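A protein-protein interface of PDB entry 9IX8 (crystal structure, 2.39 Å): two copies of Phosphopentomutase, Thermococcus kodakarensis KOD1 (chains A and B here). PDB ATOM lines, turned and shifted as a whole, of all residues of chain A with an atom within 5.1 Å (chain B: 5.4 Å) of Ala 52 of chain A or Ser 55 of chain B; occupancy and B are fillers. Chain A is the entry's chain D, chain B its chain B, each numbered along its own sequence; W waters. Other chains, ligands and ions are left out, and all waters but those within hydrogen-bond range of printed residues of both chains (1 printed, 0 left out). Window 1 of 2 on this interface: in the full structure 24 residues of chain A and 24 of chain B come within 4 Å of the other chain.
OG of Ser 55 of chain B is in hydrogen-bond range of O of Met 48 of chain A, 2.6 Å away. The side-chain sulfur (SD) of Met 48 of chain A sits close to the backbone NH (N) of Ser 59 of chain B (3.6 Å).
O of Gly 56 of chain B is in hydrogen-bond range of OG of Ser 59 of chain B, 2.7 Å away. The backbone carbonyl oxygen of Val 47 of chain A lies close to the side-chain amide oxygen of Asn 51 of chain A, at 3.1 Å.
Among the printed residues, merely in contact across the chains: Asn 51 of chain A with Ile 54 of chain B, Asn 51 of chain A with Asn 51 of chain B, Ser 55 of chain A with Ala 52 of chain B, Met 22 of chain A with Met 22 of chain B, Ile 54 of chain A with Asn 51 of chain B, Pro 18 of chain A with Met 22 of chain B, Ala 52 of chain A with Ser 55 of chain B, Pro 18 of chain A with Ser 55 of chain B, Met 48 of chain A with Leu 58 of chain B and Pro 18 of chain A with Met 26 of chain B.
Ala 52 of chain A touches one residue of chain B. Printed residues of chain B within 4 Å of Met 22 of chain A: Met 22 (3.4 Å). Of the printed residues of chain A, Ala 52 of chain B touches Ser 55. Printed residues of chain A within 4 Å of Met 22 of chain B: Pro 18 (3.5 Å) and Met 22 (3.4 Å). Of the printed residues of chain A, Ser 59 of chain B touches Met 48 (3.4 Å).
Hydrophobic or aromatic side chains of chain B that line the printed part of chain A: Met 22, Met 26, Ala 52, Ile 54 and Leu 58. Along chain B the printed residues that touch a printed residue of chain A span positions 22 to 59. Printed residues of chain A that touch a printed residue of chain B: Pro 18, Met 22, Met 48, Asn 51, Ala 52, Ile 54 and Ser 55. Among the printed residues, no Asp or Glu carboxylate lies within 4 Å of a Lys or Arg side-chain nitrogen of the other chain.
Met 22 of chain A touches its own counterpart, Met 22 of chain B. Asn 51 of chain A touches its own counterpart, Asn 51 of chain B. Asn 51 of chain A touches Ile 54 of chain B, and with the chains exchanged Ile 54 of chain A touches Asn 51 of chain B. Ala 52 of chain A touches Ser 55 of chain B, and with the chains exchanged Ser 55 of chain A touches Ala 52 of chain B. Of the 12 pairs that touch across the chains among the printed residues, 6 have their exchanged pair printed and touching as well.
Water W1 bridges OD1 of Asn 51 of chain B (2.7 Å) and OD1 of Asn 51 of chain A (3.3 Å).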
ATOM      1  N   PRO A  18      11.367  28.337 -24.989  1.00  0.00           N
ATOM      2  CA  PRO A  18      12.497  27.576 -24.468  1.00  0.00           C
ATOM      3  C   PRO A  18      13.379  28.434 -23.543  1.00  0.00           C
ATOM      4  O   PRO A  18      13.758  27.962 -22.459  1.00  0.00           O
ATOM      5  CB  PRO A  18      13.266  27.157 -25.731  1.00  0.00           C
ATOM      6  CG  PRO A  18      12.231  27.194 -26.804  1.00  0.00           C
ATOM      7  CD  PRO A  18      11.327  28.351 -26.453  1.00  0.00           C
ATOM      8  N   ALA A  21      11.748  28.879 -20.200  1.00  0.00           N
ATOM      9  CA  ALA A  21      11.725  27.590 -19.443  1.00  0.00           C
ATOM     10  C   ALA A  21      13.107  27.318 -18.860  1.00  0.00           C
ATOM     11  O   ALA A  21      13.150  26.792 -17.724  1.00  0.00           O
ATOM     12  CB  ALA A  21      11.296  26.431 -20.306  1.00  0.00           C
ATOM     13  N   MET A  22      14.166  27.615 -19.618  1.00  0.00           N
ATOM     14  CA  MET A  22      15.567  27.499 -19.121  1.00  0.00           C
ATOM     15  C   MET A  22      15.777  28.518 -17.996  1.00  0.00           C
ATOM     16  O   MET A  22      16.438  28.162 -17.013  1.00  0.00           O
ATOM     17  CB  MET A  22      16.616  27.742 -20.205  1.00  0.00           C
ATOM     18  CG  MET A  22      18.053  27.454 -19.748  1.00  0.00           C
ATOM     19  SD  MET A  22      19.222  27.473 -21.144  1.00  0.00           S
ATOM     20  CE  MET A  22      18.865  29.104 -21.779  1.00  0.00           C
ATOM     21  N   VAL A  47       7.981  18.407 -24.535  1.00  0.00           N
ATOM     22  CA  VAL A  47       9.350  17.843 -24.472  1.00  0.00           C
ATOM     23  C   VAL A  47      10.395  18.948 -24.718  1.00  0.00           C
ATOM     24  O   VAL A  47      11.476  18.954 -24.029  1.00  0.00           O
ATOM     25  CB  VAL A  47       9.504  16.673 -25.440  1.00  0.00           C
ATOM     26  CG1 VAL A  47      10.980  16.313 -25.654  1.00  0.00           C
ATOM     27  CG2 VAL A  47       8.722  15.481 -24.919  1.00  0.00           C
ATOM     28  N   MET A  48      10.106  19.859 -25.658  1.00  0.00           N
ATOM     29  CA  MET A  48      10.983  21.012 -25.989  1.00  0.00           C
ATOM     30  C   MET A  48      11.213  21.824 -24.704  1.00  0.00           C
ATOM     31  O   MET A  48      12.376  22.082 -24.378  1.00  0.00           O
ATOM     32  CB  MET A  48      10.328  21.860 -27.079  1.00  0.00           C
ATOM     33  CG  MET A  48      11.173  23.040 -27.492  1.00  0.00           C
ATOM     34  SD  MET A  48      10.369  24.136 -28.663  1.00  0.00           S
ATOM     35  CE  MET A  48       9.067  24.793 -27.627  1.00  0.00           C
ATOM     36  N   LEU A  49      10.154  22.126 -23.942  1.00  0.00           N
ATOM     37  CA  LEU A  49      10.247  23.007 -22.762  1.00  0.00           C
ATOM     38  C   LEU A  49      10.864  22.226 -21.587  1.00  0.00           C
ATOM     39  O   LEU A  49      11.537  22.837 -20.784  1.00  0.00           O
ATOM     40  CB  LEU A  49       8.847  23.533 -22.459  1.00  0.00           C
ATOM     41  CG  LEU A  49       8.225  24.396 -23.565  1.00  0.00           C
ATOM     42  CD1 LEU A  49       6.849  24.841 -23.157  1.00  0.00           C
ATOM     43  CD2 LEU A  49       9.072  25.610 -23.910  1.00  0.00           C
ATOM     44  N   LYS A  50      10.655  20.913 -21.508  1.00  0.00           N
ATOM     45  CA  LYS A  50      11.201  20.053 -20.446  1.00  0.00           C
ATOM     46  C   LYS A  50      12.716  20.010 -20.661  1.00  0.00           C
ATOM     47  O   LYS A  50      13.424  20.218 -19.677  1.00  0.00           O
ATOM     48  CB  LYS A  50      10.590  18.641 -20.477  1.00  0.00           C
ATOM     49  CG  LYS A  50      11.043  17.730 -19.345  1.00  0.00           C
ATOM     50  CD  LYS A  50      10.769  16.266 -19.501  1.00  0.00           C
ATOM     51  CE  LYS A  50      11.674  15.589 -20.501  1.00  0.00           C
ATOM     52  NZ  LYS A  50      11.578  14.097 -20.439  1.00  0.00           N
ATOM     53  N   ASN A  51      13.186  19.794 -21.902  1.00  0.00           N
ATOM     54  CA  ASN A  51      14.644  19.769 -22.203  1.00  0.00           C
ATOM     55  C   ASN A  51      15.245  21.130 -21.802  1.00  0.00           C
ATOM     56  O   ASN A  51      16.301  21.111 -21.230  1.00  0.00           O
ATOM     57  CB  ASN A  51      14.974  19.393 -23.654  1.00  0.00           C
ATOM     58  CG  ASN A  51      14.686  17.946 -24.048  1.00  0.00           C
ATOM     59  OD1 ASN A  51      13.976  17.189 -23.423  1.00  0.00           O
ATOM     60  ND2 ASN A  51      15.223  17.521 -25.137  1.00  0.00           N
ATOM     61  N   ALA A  52      14.597  22.269 -22.051  1.00  0.00           N
ATOM     62  CA  ALA A  52      15.122  23.595 -21.636  1.00  0.00           C
ATOM     63  C   ALA A  52      15.196  23.665 -20.102  1.00  0.00           C
ATOM     64  O   ALA A  52      16.197  24.138 -19.525  1.00  0.00           O
ATOM     65  CB  ALA A  52      14.259  24.712 -22.177  1.00  0.00           C
ATOM     66  N   MET A  53      14.134  23.210 -19.461  1.00  0.00           N
ATOM     67  CA  MET A  53      13.945  23.309 -18.011  1.00  0.00           C
ATOM     68  C   MET A  53      15.072  22.527 -17.353  1.00  0.00           C
ATOM     69  O   MET A  53      15.663  22.993 -16.391  1.00  0.00           O
ATOM     70  CB  MET A  53      12.580  22.726 -17.630  1.00  0.00           C
ATOM     71  CG  MET A  53      12.341  22.578 -16.149  1.00  0.00           C
ATOM     72  SD  MET A  53      12.316  24.161 -15.403  1.00  0.00           S
ATOM     73  CE  MET A  53      10.841  24.826 -16.160  1.00  0.00           C
ATOM     74  N   ILE A  54      15.312  21.339 -17.863  1.00  0.00           N
ATOM     75  CA  ILE A  54      16.310  20.394 -17.315  1.00  0.00           C
ATOM     76  C   ILE A  54      17.702  21.014 -17.506  1.00  0.00           C
ATOM     77  O   ILE A  54      18.518  20.980 -16.544  1.00  0.00           O
ATOM     78  CB  ILE A  54      16.101  19.006 -17.951  1.00  0.00           C
ATOM     79  CG1 ILE A  54      14.810  18.393 -17.395  1.00  0.00           C
ATOM     80  CG2 ILE A  54      17.316  18.111 -17.767  1.00  0.00           C
ATOM     81  CD1 ILE A  54      14.347  17.138 -18.107  1.00  0.00           C
ATOM     82  N   SER A  55      17.950  21.612 -18.668  1.00  0.00           N
ATOM     83  CA  SER A  55      19.228  22.290 -18.965  1.00  0.00           C
ATOM     84  C   SER A  55      19.499  23.354 -17.884  1.00  0.00           C
ATOM     85  O   SER A  55      20.588  23.345 -17.309  1.00  0.00           O
ATOM     86  CB  SER A  55      19.207  22.864 -20.289  1.00  0.00           C
ATOM     87  OG  SER A  55      20.516  23.209 -20.668  1.00  0.00           O
ATOM     88  N   GLY A  56      18.466  24.113 -17.535  1.00  0.00           N
ATOM     89  CA  GLY A  56      18.434  25.168 -16.501  1.00  0.00           C
ATOM     90  C   GLY A  56      18.704  24.638 -15.115  1.00  0.00           C
ATOM     91  O   GLY A  56      19.637  25.166 -14.449  1.00  0.00           O
ATOM     92  N   MET B  22      21.584  26.304 -26.949  1.00  0.00           N
ATOM     93  CA  MET B  22      20.192  26.456 -27.468  1.00  0.00           C
ATOM     94  C   MET B  22      20.202  27.343 -28.725  1.00  0.00           C
ATOM     95  O   MET B  22      19.514  27.034 -29.723  1.00  0.00           O
ATOM     96  CB  MET B  22      19.274  27.071 -26.402  1.00  0.00           C
ATOM     97  CG  MET B  22      17.869  27.359 -26.904  1.00  0.00           C
ATOM     98  SD  MET B  22      16.688  27.758 -25.573  1.00  0.00           S
ATOM     99  CE  MET B  22      17.485  29.197 -24.860  1.00  0.00           C
ATOM    100  N   MET B  26      18.933  26.453 -32.415  1.00  0.00           N
ATOM    101  CA  MET B  26      17.980  27.340 -33.126  1.00  0.00           C
ATOM    102  C   MET B  26      18.565  27.781 -34.479  1.00  0.00           C
ATOM    103  O   MET B  26      17.842  27.660 -35.480  1.00  0.00           O
ATOM    104  CB  MET B  26      17.608  28.540 -32.264  1.00  0.00           C
ATOM    105  CG  MET B  26      16.642  28.147 -31.200  1.00  0.00           C
ATOM    106  SD  MET B  26      16.229  29.550 -30.152  1.00  0.00           S
ATOM    107  CE  MET B  26      14.991  28.823 -29.082  1.00  0.00           C
ATOM    108  N   LYS B  50      23.307  19.190 -24.222  1.00  0.00           N
ATOM    109  CA  LYS B  50      22.524  18.381 -25.185  1.00  0.00           C
ATOM    110  C   LYS B  50      21.036  18.742 -25.000  1.00  0.00           C
ATOM    111  O   LYS B  50      20.350  19.016 -25.987  1.00  0.00           O
ATOM    112  CB  LYS B  50      22.776  16.877 -24.982  1.00  0.00           C
ATOM    113  CG  LYS B  50      22.180  15.993 -26.079  1.00  0.00           C
ATOM    114  CD  LYS B  50      22.075  14.551 -25.713  1.00  0.00           C
ATOM    115  CE  LYS B  50      20.960  14.291 -24.709  1.00  0.00           C
ATOM    116  NZ  LYS B  50      20.637  12.848 -24.549  1.00  0.00           N
ATOM    117  N   ASN B  51      20.568  18.768 -23.756  1.00  0.00           N
ATOM    118  CA  ASN B  51      19.188  19.176 -23.435  1.00  0.00           C
ATOM    119  C   ASN B  51      18.908  20.542 -24.052  1.00  0.00           C
ATOM    120  O   ASN B  51      17.810  20.704 -24.596  1.00  0.00           O
ATOM    121  CB  ASN B  51      18.924  19.111 -21.947  1.00  0.00           C
ATOM    122  CG  ASN B  51      18.464  17.721 -21.537  1.00  0.00           C
ATOM    123  OD1 ASN B  51      17.315  17.520 -21.150  1.00  0.00           O
ATOM    124  ND2 ASN B  51      19.316  16.741 -21.688  1.00  0.00           N
ATOM    125  N   ALA B  52      19.860  21.482 -23.985  1.00  0.00           N
ATOM    126  CA  ALA B  52      19.628  22.882 -24.415  1.00  0.00           C
ATOM    127  C   ALA B  52      19.577  22.897 -25.942  1.00  0.00           C
ATOM    128  O   ALA B  52      18.608  23.415 -26.471  1.00  0.00           O
ATOM    129  CB  ALA B  52      20.700  23.793 -23.889  1.00  0.00           C
ATOM    130  N   MET B  53      20.571  22.253 -26.573  1.00  0.00           N
ATOM    131  CA  MET B  53      20.707  22.040 -28.028  1.00  0.00           C
ATOM    132  C   MET B  53      19.393  21.505 -28.594  1.00  0.00           C
ATOM    133  O   MET B  53      18.938  21.959 -29.676  1.00  0.00           O
ATOM    134  CB  MET B  53      21.831  21.028 -28.300  1.00  0.00           C
ATOM    135  CG  MET B  53      22.007  20.678 -29.785  1.00  0.00           C
ATOM    136  SD  MET B  53      22.329  22.179 -30.754  1.00  0.00           S
ATOM    137  CE  MET B  53      23.869  22.669 -29.984  1.00  0.00           C
ATOM    138  N   ILE B  54      18.843  20.491 -27.935  1.00  0.00           N
ATOM    139  CA  ILE B  54      17.737  19.670 -28.502  1.00  0.00           C
ATOM    140  C   ILE B  54      16.476  20.536 -28.484  1.00  0.00           C
ATOM    141  O   ILE B  54      15.725  20.511 -29.481  1.00  0.00           O
ATOM    142  CB  ILE B  54      17.597  18.318 -27.761  1.00  0.00           C
ATOM    143  CG1 ILE B  54      18.677  17.330 -28.251  1.00  0.00           C
ATOM    144  CG2 ILE B  54      16.184  17.738 -27.913  1.00  0.00           C
ATOM    145  CD1 ILE B  54      18.656  15.983 -27.527  1.00  0.00           C
ATOM    146  N   SER B  55      16.306  21.299 -27.412  1.00  0.00           N
ATOM    147  CA  SER B  55      15.262  22.330 -27.240  1.00  0.00           C
ATOM    148  C   SER B  55      15.330  23.293 -28.411  1.00  0.00           C
ATOM    149  O   SER B  55      14.314  23.508 -29.040  1.00  0.00           O
ATOM    150  CB  SER B  55      15.423  23.037 -25.960  1.00  0.00           C
ATOM    151  OG  SER B  55      14.187  23.591 -25.541  1.00  0.00           O
ATOM    152  N   GLY B  56      16.522  23.798 -28.692  1.00  0.00           N
ATOM    153  CA  GLY B  56      16.827  24.635 -29.867  1.00  0.00           C
ATOM    154  C   GLY B  56      16.333  24.003 -31.142  1.00  0.00           C
ATOM    155  O   GLY B  56      15.435  24.612 -31.793  1.00  0.00           O
ATOM    156  N   LEU B  57      16.887  22.832 -31.469  1.00  0.00           N
ATOM    157  CA  LEU B  57      16.542  22.117 -32.714  1.00  0.00           C
ATOM    158  C   LEU B  57      15.012  21.972 -32.807  1.00  0.00           C
ATOM    159  O   LEU B  57      14.428  22.448 -33.813  1.00  0.00           O
ATOM    160  CB  LEU B  57      17.307  20.785 -32.748  1.00  0.00           C
ATOM    161  CG  LEU B  57      18.836  20.885 -32.909  1.00  0.00           C
ATOM    162  CD1 LEU B  57      19.538  19.546 -32.735  1.00  0.00           C
ATOM    163  CD2 LEU B  57      19.204  21.451 -34.263  1.00  0.00           C
ATOM    164  N   LEU B  58      14.365  21.473 -31.749  1.00  0.00           N
ATOM    165  CA  LEU B  58      12.902  21.179 -31.779  1.00  0.00           C
ATOM    166  C   LEU B  58      12.101  22.436 -32.130  1.00  0.00           C
ATOM    167  O   LEU B  58      11.071  22.277 -32.810  1.00  0.00           O
ATOM    168  CB  LEU B  58      12.427  20.647 -30.417  1.00  0.00           C
ATOM    169  CG  LEU B  58      12.854  19.219 -30.087  1.00  0.00           C
ATOM    170  CD1 LEU B  58      12.403  18.863 -28.679  1.00  0.00           C
ATOM    171  CD2 LEU B  58      12.301  18.226 -31.116  1.00  0.00           C
ATOM    172  N   SER B  59      12.476  23.591 -31.552  1.00  0.00           N
ATOM    173  CA  SER B  59      11.803  24.912 -31.690  1.00  0.00           C
ATOM    174  C   SER B  59      11.721  25.388 -33.151  1.00  0.00           C
ATOM    175  O   SER B  59      10.918  26.279 -33.409  1.00  0.00           O
ATOM    176  CB  SER B  59      12.527  25.950 -30.895  1.00  0.00           C
ATOM    177  OG  SER B  59      13.584  26.512 -31.655  1.00  0.00           O
HETATM  178  O   HOH W   1      15.635  15.441 -21.179  1.00  0.00           O
